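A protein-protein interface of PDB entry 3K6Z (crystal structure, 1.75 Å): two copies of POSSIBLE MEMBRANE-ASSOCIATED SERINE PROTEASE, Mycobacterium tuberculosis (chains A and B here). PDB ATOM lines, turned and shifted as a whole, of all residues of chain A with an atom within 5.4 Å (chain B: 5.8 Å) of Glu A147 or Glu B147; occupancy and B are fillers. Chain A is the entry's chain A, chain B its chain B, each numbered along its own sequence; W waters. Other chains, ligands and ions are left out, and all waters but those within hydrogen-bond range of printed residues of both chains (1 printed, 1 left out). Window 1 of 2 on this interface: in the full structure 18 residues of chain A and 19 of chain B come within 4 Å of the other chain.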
ATOM      1  N   HIS A  57     -15.617 -13.550  -9.931  1.00  0.00           N
ATOM      2  CA  HIS A  57     -15.425 -14.765 -10.735  1.00  0.00           C
ATOM      3  C   HIS A  57     -16.660 -15.645 -10.879  1.00  0.00           C
ATOM      4  O   HIS A  57     -16.754 -16.446 -11.819  1.00  0.00           O
ATOM      5  CB  HIS A  57     -14.250 -15.564 -10.190  1.00  0.00           C
ATOM      6  CG  HIS A  57     -12.962 -14.814 -10.234  1.00  0.00           C
ATOM      7  ND1 HIS A  57     -12.308 -14.537 -11.416  1.00  0.00           N
ATOM      8  CD2 HIS A  57     -12.223 -14.250  -9.253  1.00  0.00           C
ATOM      9  CE1 HIS A  57     -11.211 -13.849 -11.158  1.00  0.00           C
ATOM     10  NE2 HIS A  57     -11.133 -13.665  -9.854  1.00  0.00           N
ATOM     11  N   PRO A  83     -12.376  -6.713 -14.669  1.00  0.00           N
ATOM     12  CA  PRO A  83     -11.463  -7.856 -14.550  1.00  0.00           C
ATOM     13  C   PRO A  83     -10.330  -7.659 -13.534  1.00  0.00           C
ATOM     14  O   PRO A  83      -9.779  -8.641 -13.046  1.00  0.00           O
ATOM     15  CB  PRO A  83     -10.904  -8.004 -15.970  1.00  0.00           C
ATOM     16  CG  PRO A  83     -11.949  -7.427 -16.835  1.00  0.00           C
ATOM     17  CD  PRO A  83     -12.506  -6.269 -16.067  1.00  0.00           C
ATOM     18  N   SER A  84     -10.009  -6.410 -13.202  1.00  0.00           N
ATOM     19  CA  SER A  84      -8.948  -6.113 -12.232  1.00  0.00           C
ATOM     20  C   SER A  84      -9.400  -6.179 -10.765  1.00  0.00           C
ATOM     21  O   SER A  84      -8.581  -6.038  -9.861  1.00  0.00           O
ATOM     22  CB  SER A  84      -8.344  -4.725 -12.511  1.00  0.00           C
ATOM     23  OG  SER A  84      -9.289  -3.699 -12.233  1.00  0.00           O
ATOM     24  N   ASP A  86     -11.722  -8.086  -7.575  1.00  0.00           N
ATOM     25  CA  ASP A  86     -12.124  -9.434  -7.116  1.00  0.00           C
ATOM     26  C   ASP A  86     -13.594  -9.558  -6.711  1.00  0.00           C
ATOM     27  O   ASP A  86     -14.121 -10.679  -6.592  1.00  0.00           O
ATOM     28  CB  ASP A  86     -11.283  -9.864  -5.914  1.00  0.00           C
ATOM     29  CG  ASP A  86      -9.821 -10.045  -6.250  1.00  0.00           C
ATOM     30  OD1 ASP A  86      -8.984  -9.478  -5.510  1.00  0.00           O
ATOM     31  OD2 ASP A  86      -9.516 -10.739  -7.244  1.00  0.00           O
ATOM     32  N   ILE A 142       2.125 -12.078 -13.189  1.00  0.00           N
ATOM     33  CA  ILE A 142       1.709 -12.857 -14.342  1.00  0.00           C
ATOM     34  C   ILE A 142       1.358 -11.877 -15.455  1.00  0.00           C
ATOM     35  O   ILE A 142       0.381 -11.136 -15.355  1.00  0.00           O
ATOM     36  CB  ILE A 142       0.498 -13.781 -14.006  1.00  0.00           C
ATOM     37  CG1 ILE A 142       0.808 -14.694 -12.802  1.00  0.00           C
ATOM     38  CG2 ILE A 142       0.042 -14.571 -15.240  1.00  0.00           C
ATOM     39  CD1 ILE A 142       2.060 -15.552 -12.925  1.00  0.00           C
ATOM     40  N   ASP A 145      -2.275 -10.601 -16.796  1.00  0.00           N
ATOM     41  CA  ASP A 145      -3.291 -10.936 -15.811  1.00  0.00           C
ATOM     42  C   ASP A 145      -3.705  -9.634 -15.117  1.00  0.00           C
ATOM     43  O   ASP A 145      -2.884  -9.021 -14.429  1.00  0.00           O
ATOM     44  CB  ASP A 145      -2.729 -11.945 -14.802  1.00  0.00           C
ATOM     45  CG  ASP A 145      -3.772 -12.453 -13.809  1.00  0.00           C
ATOM     46  OD1 ASP A 145      -4.888 -11.903 -13.743  1.00  0.00           O
ATOM     47  OD2 ASP A 145      -3.456 -13.414 -13.073  1.00  0.00           O
ATOM     48  N   PRO A 146      -4.973  -9.204 -15.305  1.00  0.00           N
ATOM     49  CA  PRO A 146      -5.412  -7.899 -14.788  1.00  0.00           C
ATOM     50  C   PRO A 146      -5.643  -7.852 -13.272  1.00  0.00           C
ATOM     51  O   PRO A 146      -5.699  -6.758 -12.691  1.00  0.00           O
ATOM     52  CB  PRO A 146      -6.727  -7.648 -15.542  1.00  0.00           C
ATOM     53  CG  PRO A 146      -7.255  -9.002 -15.846  1.00  0.00           C
ATOM     54  CD  PRO A 146      -6.057  -9.914 -16.011  1.00  0.00           C
ATOM     55  N   GLU A 147      -5.759  -9.020 -12.639  1.00  0.00           N
ATOM     56  CA  GLU A 147      -6.028  -9.081 -11.202  1.00  0.00           C
ATOM     57  C   GLU A 147      -4.882  -8.519 -10.348  1.00  0.00           C
ATOM     58  O   GLU A 147      -3.737  -8.463 -10.803  1.00  0.00           O
ATOM     59  CB  GLU A 147      -6.436 -10.503 -10.773  1.00  0.00           C
ATOM     60  CG  GLU A 147      -5.344 -11.555 -10.748  1.00  0.00           C
ATOM     61  CD  GLU A 147      -5.903 -12.979 -10.644  1.00  0.00           C
ATOM     62  OE1 GLU A 147      -7.088 -13.132 -10.252  1.00  0.00           O
ATOM     63  OE2 GLU A 147      -5.159 -13.942 -10.956  1.00  0.00           O
ATOM     64  N   PRO A 148      -5.192  -8.080  -9.113  1.00  0.00           N
ATOM     65  CA  PRO A 148      -4.160  -7.536  -8.231  1.00  0.00           C
ATOM     66  C   PRO A 148      -3.039  -8.540  -7.972  1.00  0.00           C
ATOM     67  O   PRO A 148      -3.302  -9.733  -7.779  1.00  0.00           O
ATOM     68  CB  PRO A 148      -4.926  -7.262  -6.926  1.00  0.00           C
ATOM     69  CG  PRO A 148      -6.338  -7.103  -7.347  1.00  0.00           C
ATOM     70  CD  PRO A 148      -6.523  -8.060  -8.471  1.00  0.00           C
ATOM     71  N   VAL A 149      -1.801  -8.053  -7.986  1.00  0.00           N
ATOM     72  CA  VAL A 149      -0.639  -8.873  -7.651  1.00  0.00           C
ATOM     73  C   VAL A 149      -0.596  -9.121  -6.139  1.00  0.00           C
ATOM     74  O   VAL A 149      -0.186 -10.200  -5.695  1.00  0.00           O
ATOM     75  CB  VAL A 149       0.692  -8.229  -8.155  1.00  0.00           C
ATOM     76  CG1 VAL A 149       1.905  -8.946  -7.595  1.00  0.00           C
ATOM     77  CG2 VAL A 149       0.755  -8.253  -9.678  1.00  0.00           C
ATOM     78  N   ARG A 151      -2.879  -8.475  -2.284  1.00  0.00           N
ATOM     79  CA  ARG A 151      -4.177  -8.216  -1.663  1.00  0.00           C
ATOM     80  C   ARG A 151      -4.015  -8.316  -0.152  1.00  0.00           C
ATOM     81  O   ARG A 151      -3.282  -9.179   0.335  1.00  0.00           O
ATOM     82  CB  ARG A 151      -5.198  -9.267  -2.102  1.00  0.00           C
ATOM     83  CG  ARG A 151      -5.523  -9.328  -3.586  1.00  0.00           C
ATOM     84  CD  ARG A 151      -6.108 -10.698  -3.880  1.00  0.00           C
ATOM     85  NE  ARG A 151      -6.658 -10.857  -5.223  1.00  0.00           N
ATOM     86  CZ  ARG A 151      -6.090 -11.571  -6.191  1.00  0.00           C
ATOM     87  NH1 ARG A 151      -4.923 -12.179  -5.984  1.00  0.00           N
ATOM     88  NH2 ARG A 151      -6.687 -11.680  -7.370  1.00  0.00           N
ATOM     89  N   HIS B  57      -3.304 -13.977 -22.735  1.00  0.00           N
ATOM     90  CA  HIS B  57      -3.645 -12.623 -22.277  1.00  0.00           C
ATOM     91  C   HIS B  57      -3.379 -11.525 -23.294  1.00  0.00           C
ATOM     92  O   HIS B  57      -3.902 -10.423 -23.167  1.00  0.00           O
ATOM     93  CB  HIS B  57      -2.910 -12.293 -20.985  1.00  0.00           C
ATOM     94  CG  HIS B  57      -3.381 -13.088 -19.817  1.00  0.00           C
ATOM     95  ND1 HIS B  57      -2.676 -14.158 -19.311  1.00  0.00           N
ATOM     96  CD2 HIS B  57      -4.506 -12.990 -19.073  1.00  0.00           C
ATOM     97  CE1 HIS B  57      -3.340 -14.674 -18.293  1.00  0.00           C
ATOM     98  NE2 HIS B  57      -4.455 -13.986 -18.131  1.00  0.00           N
ATOM     99  N   PRO B  83      -9.784 -19.436 -21.226  1.00  0.00           N
ATOM    100  CA  PRO B  83      -9.356 -18.612 -20.091  1.00  0.00           C
ATOM    101  C   PRO B  83      -8.542 -19.367 -19.026  1.00  0.00           C
ATOM    102  O   PRO B  83      -7.799 -18.736 -18.278  1.00  0.00           O
ATOM    103  CB  PRO B  83     -10.683 -18.121 -19.494  1.00  0.00           C
ATOM    104  CG  PRO B  83     -11.652 -18.199 -20.617  1.00  0.00           C
ATOM    105  CD  PRO B  83     -11.249 -19.408 -21.403  1.00  0.00           C
ATOM    106  N   SER B  84      -8.670 -20.690 -18.955  1.00  0.00           N
ATOM    107  CA  SER B  84      -7.942 -21.469 -17.948  1.00  0.00           C
ATOM    108  C   SER B  84      -6.514 -21.799 -18.386  1.00  0.00           C
ATOM    109  O   SER B  84      -5.766 -22.442 -17.648  1.00  0.00           O
ATOM    110  CB  SER B  84      -8.685 -22.763 -17.618  1.00  0.00           C
ATOM    111  OG  SER B  84      -8.580 -23.692 -18.686  1.00  0.00           O
ATOM    112  N   ASP B  86      -2.724 -20.553 -20.244  1.00  0.00           N
ATOM    113  CA  ASP B  86      -1.806 -19.413 -20.445  1.00  0.00           C
ATOM    114  C   ASP B  86      -1.435 -19.151 -21.901  1.00  0.00           C
ATOM    115  O   ASP B  86      -1.089 -18.021 -22.257  1.00  0.00           O
ATOM    116  CB  ASP B  86      -0.508 -19.608 -19.659  1.00  0.00           C
ATOM    117  CG  ASP B  86      -0.741 -19.745 -18.179  1.00  0.00           C
ATOM    118  OD1 ASP B  86      -0.291 -20.763 -17.617  1.00  0.00           O
ATOM    119  OD2 ASP B  86      -1.375 -18.848 -17.574  1.00  0.00           O
ATOM    120  N   ILE B 142      -7.841 -19.517  -5.803  1.00  0.00           N
ATOM    121  CA  ILE B 142      -8.760 -18.380  -5.868  1.00  0.00           C
ATOM    122  C   ILE B 142     -10.034 -18.887  -6.517  1.00  0.00           C
ATOM    123  O   ILE B 142     -10.046 -19.242  -7.694  1.00  0.00           O
ATOM    124  CB  ILE B 142      -8.176 -17.172  -6.662  1.00  0.00           C
ATOM    125  CG1 ILE B 142      -6.766 -16.803  -6.175  1.00  0.00           C
ATOM    126  CG2 ILE B 142      -9.145 -15.978  -6.650  1.00  0.00           C
ATOM    127  CD1 ILE B 142      -6.629 -16.495  -4.704  1.00  0.00           C
ATOM    128  N   ASP B 145     -11.446 -18.399 -10.221  1.00  0.00           N
ATOM    129  CA  ASP B 145     -10.396 -17.782 -11.027  1.00  0.00           C
ATOM    130  C   ASP B 145      -9.942 -18.768 -12.102  1.00  0.00           C
ATOM    131  O   ASP B 145      -9.573 -19.902 -11.781  1.00  0.00           O
ATOM    132  CB  ASP B 145      -9.213 -17.393 -10.139  1.00  0.00           C
ATOM    133  CG  ASP B 145      -8.218 -16.469 -10.825  1.00  0.00           C
ATOM    134  OD1 ASP B 145      -8.165 -16.412 -12.071  1.00  0.00           O
ATOM    135  OD2 ASP B 145      -7.457 -15.804 -10.095  1.00  0.00           O
ATOM    136  N   PRO B 146     -10.000 -18.346 -13.381  1.00  0.00           N
ATOM    137  CA  PRO B 146      -9.561 -19.155 -14.523  1.00  0.00           C
ATOM    138  C   PRO B 146      -8.142 -19.720 -14.415  1.00  0.00           C
ATOM    139  O   PRO B 146      -7.963 -20.932 -14.583  1.00  0.00           O
ATOM    140  CB  PRO B 146      -9.676 -18.185 -15.713  1.00  0.00           C
ATOM    141  CG  PRO B 146      -9.832 -16.831 -15.123  1.00  0.00           C
ATOM    142  CD  PRO B 146     -10.534 -17.046 -13.827  1.00  0.00           C
ATOM    143  N   GLU B 147      -7.162 -18.856 -14.131  1.00  0.00           N
ATOM    144  CA  GLU B 147      -5.737 -19.225 -14.078  1.00  0.00           C
ATOM    145  C   GLU B 147      -5.504 -20.600 -13.437  1.00  0.00           C
ATOM    146  O   GLU B 147      -6.186 -20.955 -12.478  1.00  0.00           O
ATOM    147  CB  GLU B 147      -4.937 -18.168 -13.302  1.00  0.00           C
ATOM    148  CG  GLU B 147      -5.107 -16.714 -13.773  1.00  0.00           C
ATOM    149  CD  GLU B 147      -4.233 -16.345 -14.973  1.00  0.00           C
ATOM    150  OE1 GLU B 147      -4.728 -15.626 -15.866  1.00  0.00           O
ATOM    151  OE2 GLU B 147      -3.053 -16.757 -15.027  1.00  0.00           O
ATOM    152  N   PRO B 148      -4.550 -21.391 -13.972  1.00  0.00           N
ATOM    153  CA  PRO B 148      -4.218 -22.631 -13.257  1.00  0.00           C
ATOM    154  C   PRO B 148      -3.688 -22.348 -11.848  1.00  0.00           C
ATOM    155  O   PRO B 148      -2.994 -21.350 -11.645  1.00  0.00           O
ATOM    156  CB  PRO B 148      -3.117 -23.270 -14.118  1.00  0.00           C
ATOM    157  CG  PRO B 148      -2.649 -22.205 -15.053  1.00  0.00           C
ATOM    158  CD  PRO B 148      -3.773 -21.229 -15.216  1.00  0.00           C
ATOM    159  N   VAL B 149      -4.023 -23.210 -10.891  1.00  0.00           N
ATOM    160  CA  VAL B 149      -3.511 -23.077  -9.517  1.00  0.00           C
ATOM    161  C   VAL B 149      -2.022 -23.444  -9.431  1.00  0.00           C
ATOM    162  O   VAL B 149      -1.262 -22.849  -8.659  1.00  0.00           O
ATOM    163  CB  VAL B 149      -4.339 -23.912  -8.494  1.00  0.00           C
ATOM    164  CG1 VAL B 149      -4.364 -25.400  -8.869  1.00  0.00           C
ATOM    165  CG2 VAL B 149      -3.793 -23.735  -7.087  1.00  0.00           C
ATOM    166  N   ARG B 151       1.551 -24.684 -11.776  1.00  0.00           N
ATOM    167  CA  ARG B 151       2.241 -24.761 -13.072  1.00  0.00           C
ATOM    168  C   ARG B 151       3.657 -25.279 -12.856  1.00  0.00           C
ATOM    169  O   ARG B 151       4.285 -24.936 -11.858  1.00  0.00           O
ATOM    170  CB  ARG B 151       2.316 -23.374 -13.719  1.00  0.00           C
ATOM    171  CG  ARG B 151       0.992 -22.828 -14.270  1.00  0.00           C
ATOM    172  CD  ARG B 151       1.147 -21.390 -14.764  1.00  0.00           C
ATOM    173  NE  ARG B 151       0.993 -20.442 -13.675  1.00  0.00           N
ATOM    174  CZ  ARG B 151       0.057 -19.499 -13.594  1.00  0.00           C
ATOM    175  NH1 ARG B 151      -0.826 -19.303 -14.570  1.00  0.00           N
ATOM    176  NH2 ARG B 151       0.038 -18.719 -12.535  1.00  0.00           N
HETATM  177  O   HOH W   1      -6.908 -13.693 -15.770  1.00  0.00           O
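His A57 touches Asp B145, and with the chains exchanged Asp A145 touches His B57. His A57 touches Pro B146, but with the chains exchanged Pro A146 does not touch His B57 (4.6 Å). Ile A142 touches Glu B147, but with the chains exchanged Glu A147 does not touch Ile B142 (5.0 Å). Asp A145 touches Glu B147, and with the chains exchanged Glu A147 touches Asp B145. Positions printed for both chains: 57, 83, 84, 86, 142, 145, 146, 147, 148, 149 and 151. Of the 8 pairs that touch across the chains among the printed residues, 5 have their exchanged pair printed and touching as well.
Water W1 lies within hydrogen-bond range of the side-chain carboxylate of Glu B147 (2.9 Å), the side-chain carboxylate of Asp A145 (3.4 Å) and a ring nitrogen (NE2) of His B57 (3.4 Å).
Of the 11 printed residues of chain A, 4 touch a printed residue of chain B. Printed residues of chain A that touch a printed residue of chain B: His A57, Ile A142, Asp A145 and Glu A147. Hydrophobic or aromatic side chains of chain A that line the printed part of chain B: His A57 and Ile A142. Along chain A the printed residues that touch a printed residue of chain B span positions 57 to 147. Of the 11 printed residues of chain B, 5 touch a printed residue of chain A. Among the printed residues, no Asp or Glu carboxylate lies within 4 Å of a Lys or Arg side-chain nitrogen of the other chain.
Of the printed residues of chain B, His A57 touches Asp B145 (3.8 Å) and Pro B146 (3.9 Å). Of the printed residues of chain B, Ile A142 touches Glu B147 and Arg B151. Glu A147 touches just these residues of chain B: Asp B145 (2.7 Å) and Glu B147 (3.95 Å). Of the printed residues of chain A, His B57 touches Asp A145 (3.98 Å). Of the printed residues of chain A, Pro B146 touches His A57. Of chain A, only Ile A142 (3.8 Å), Asp A145 (3.6 Å) and Glu A147 (3.95 Å) come within 4 Å of Glu B147. Printed residues of chain A within 4 Å of Arg B151: Ile A142 (3.8 Å). The nearest residue of chain B that does not touch Glu A147 is Ile B142 (5.0 Å). The nearest printed residue of chain A that does not touch Glu B147 is Pro A146 (5.9 Å).
OD1 of Asp A145 sits close to N of Glu A147 (3.2 Å). The side-chain carboxylate (OE1) of Glu A147 lies within salt-bridge range of the guanidinium group (NH2) of Arg A151, 3.3 Å away. OE1 of Glu B147 lies within hydrogen-bond range of NE2 of His B57. The side-chain carboxylate (OD2) of Asp B86 lies within salt-bridge range of the guanidinium group (NH1) of Arg B151 (3.1 Å). OD1 of Asp B145 lies within hydrogen-bond range of N of Glu B147, 3.4 Å away. The side-chain carboxylate (OE2) of Glu B147 is in salt-bridge range of the guanidinium group (NH1) of Arg B151 (3.4 Å).
His A57 touches Asp B145. His A57 touches Pro B146 (ND1 to CD, 3.9 Å). Ile A142 touches Glu B147. CD1 of Ile A142 touches NH2 of Arg B151 (3.8 Å). His B57 touches Asp A145 (CD2 to N, 3.98 Å). Glu B147 touches Asp A145. Glu A147 touches Glu B147 (OE2 to CG, 3.95 Å).
The side-chain carboxylate (OE1) of Glu A147 lies close to the side-chain carboxylate (OD2) of Asp B145 (2.7 Å).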
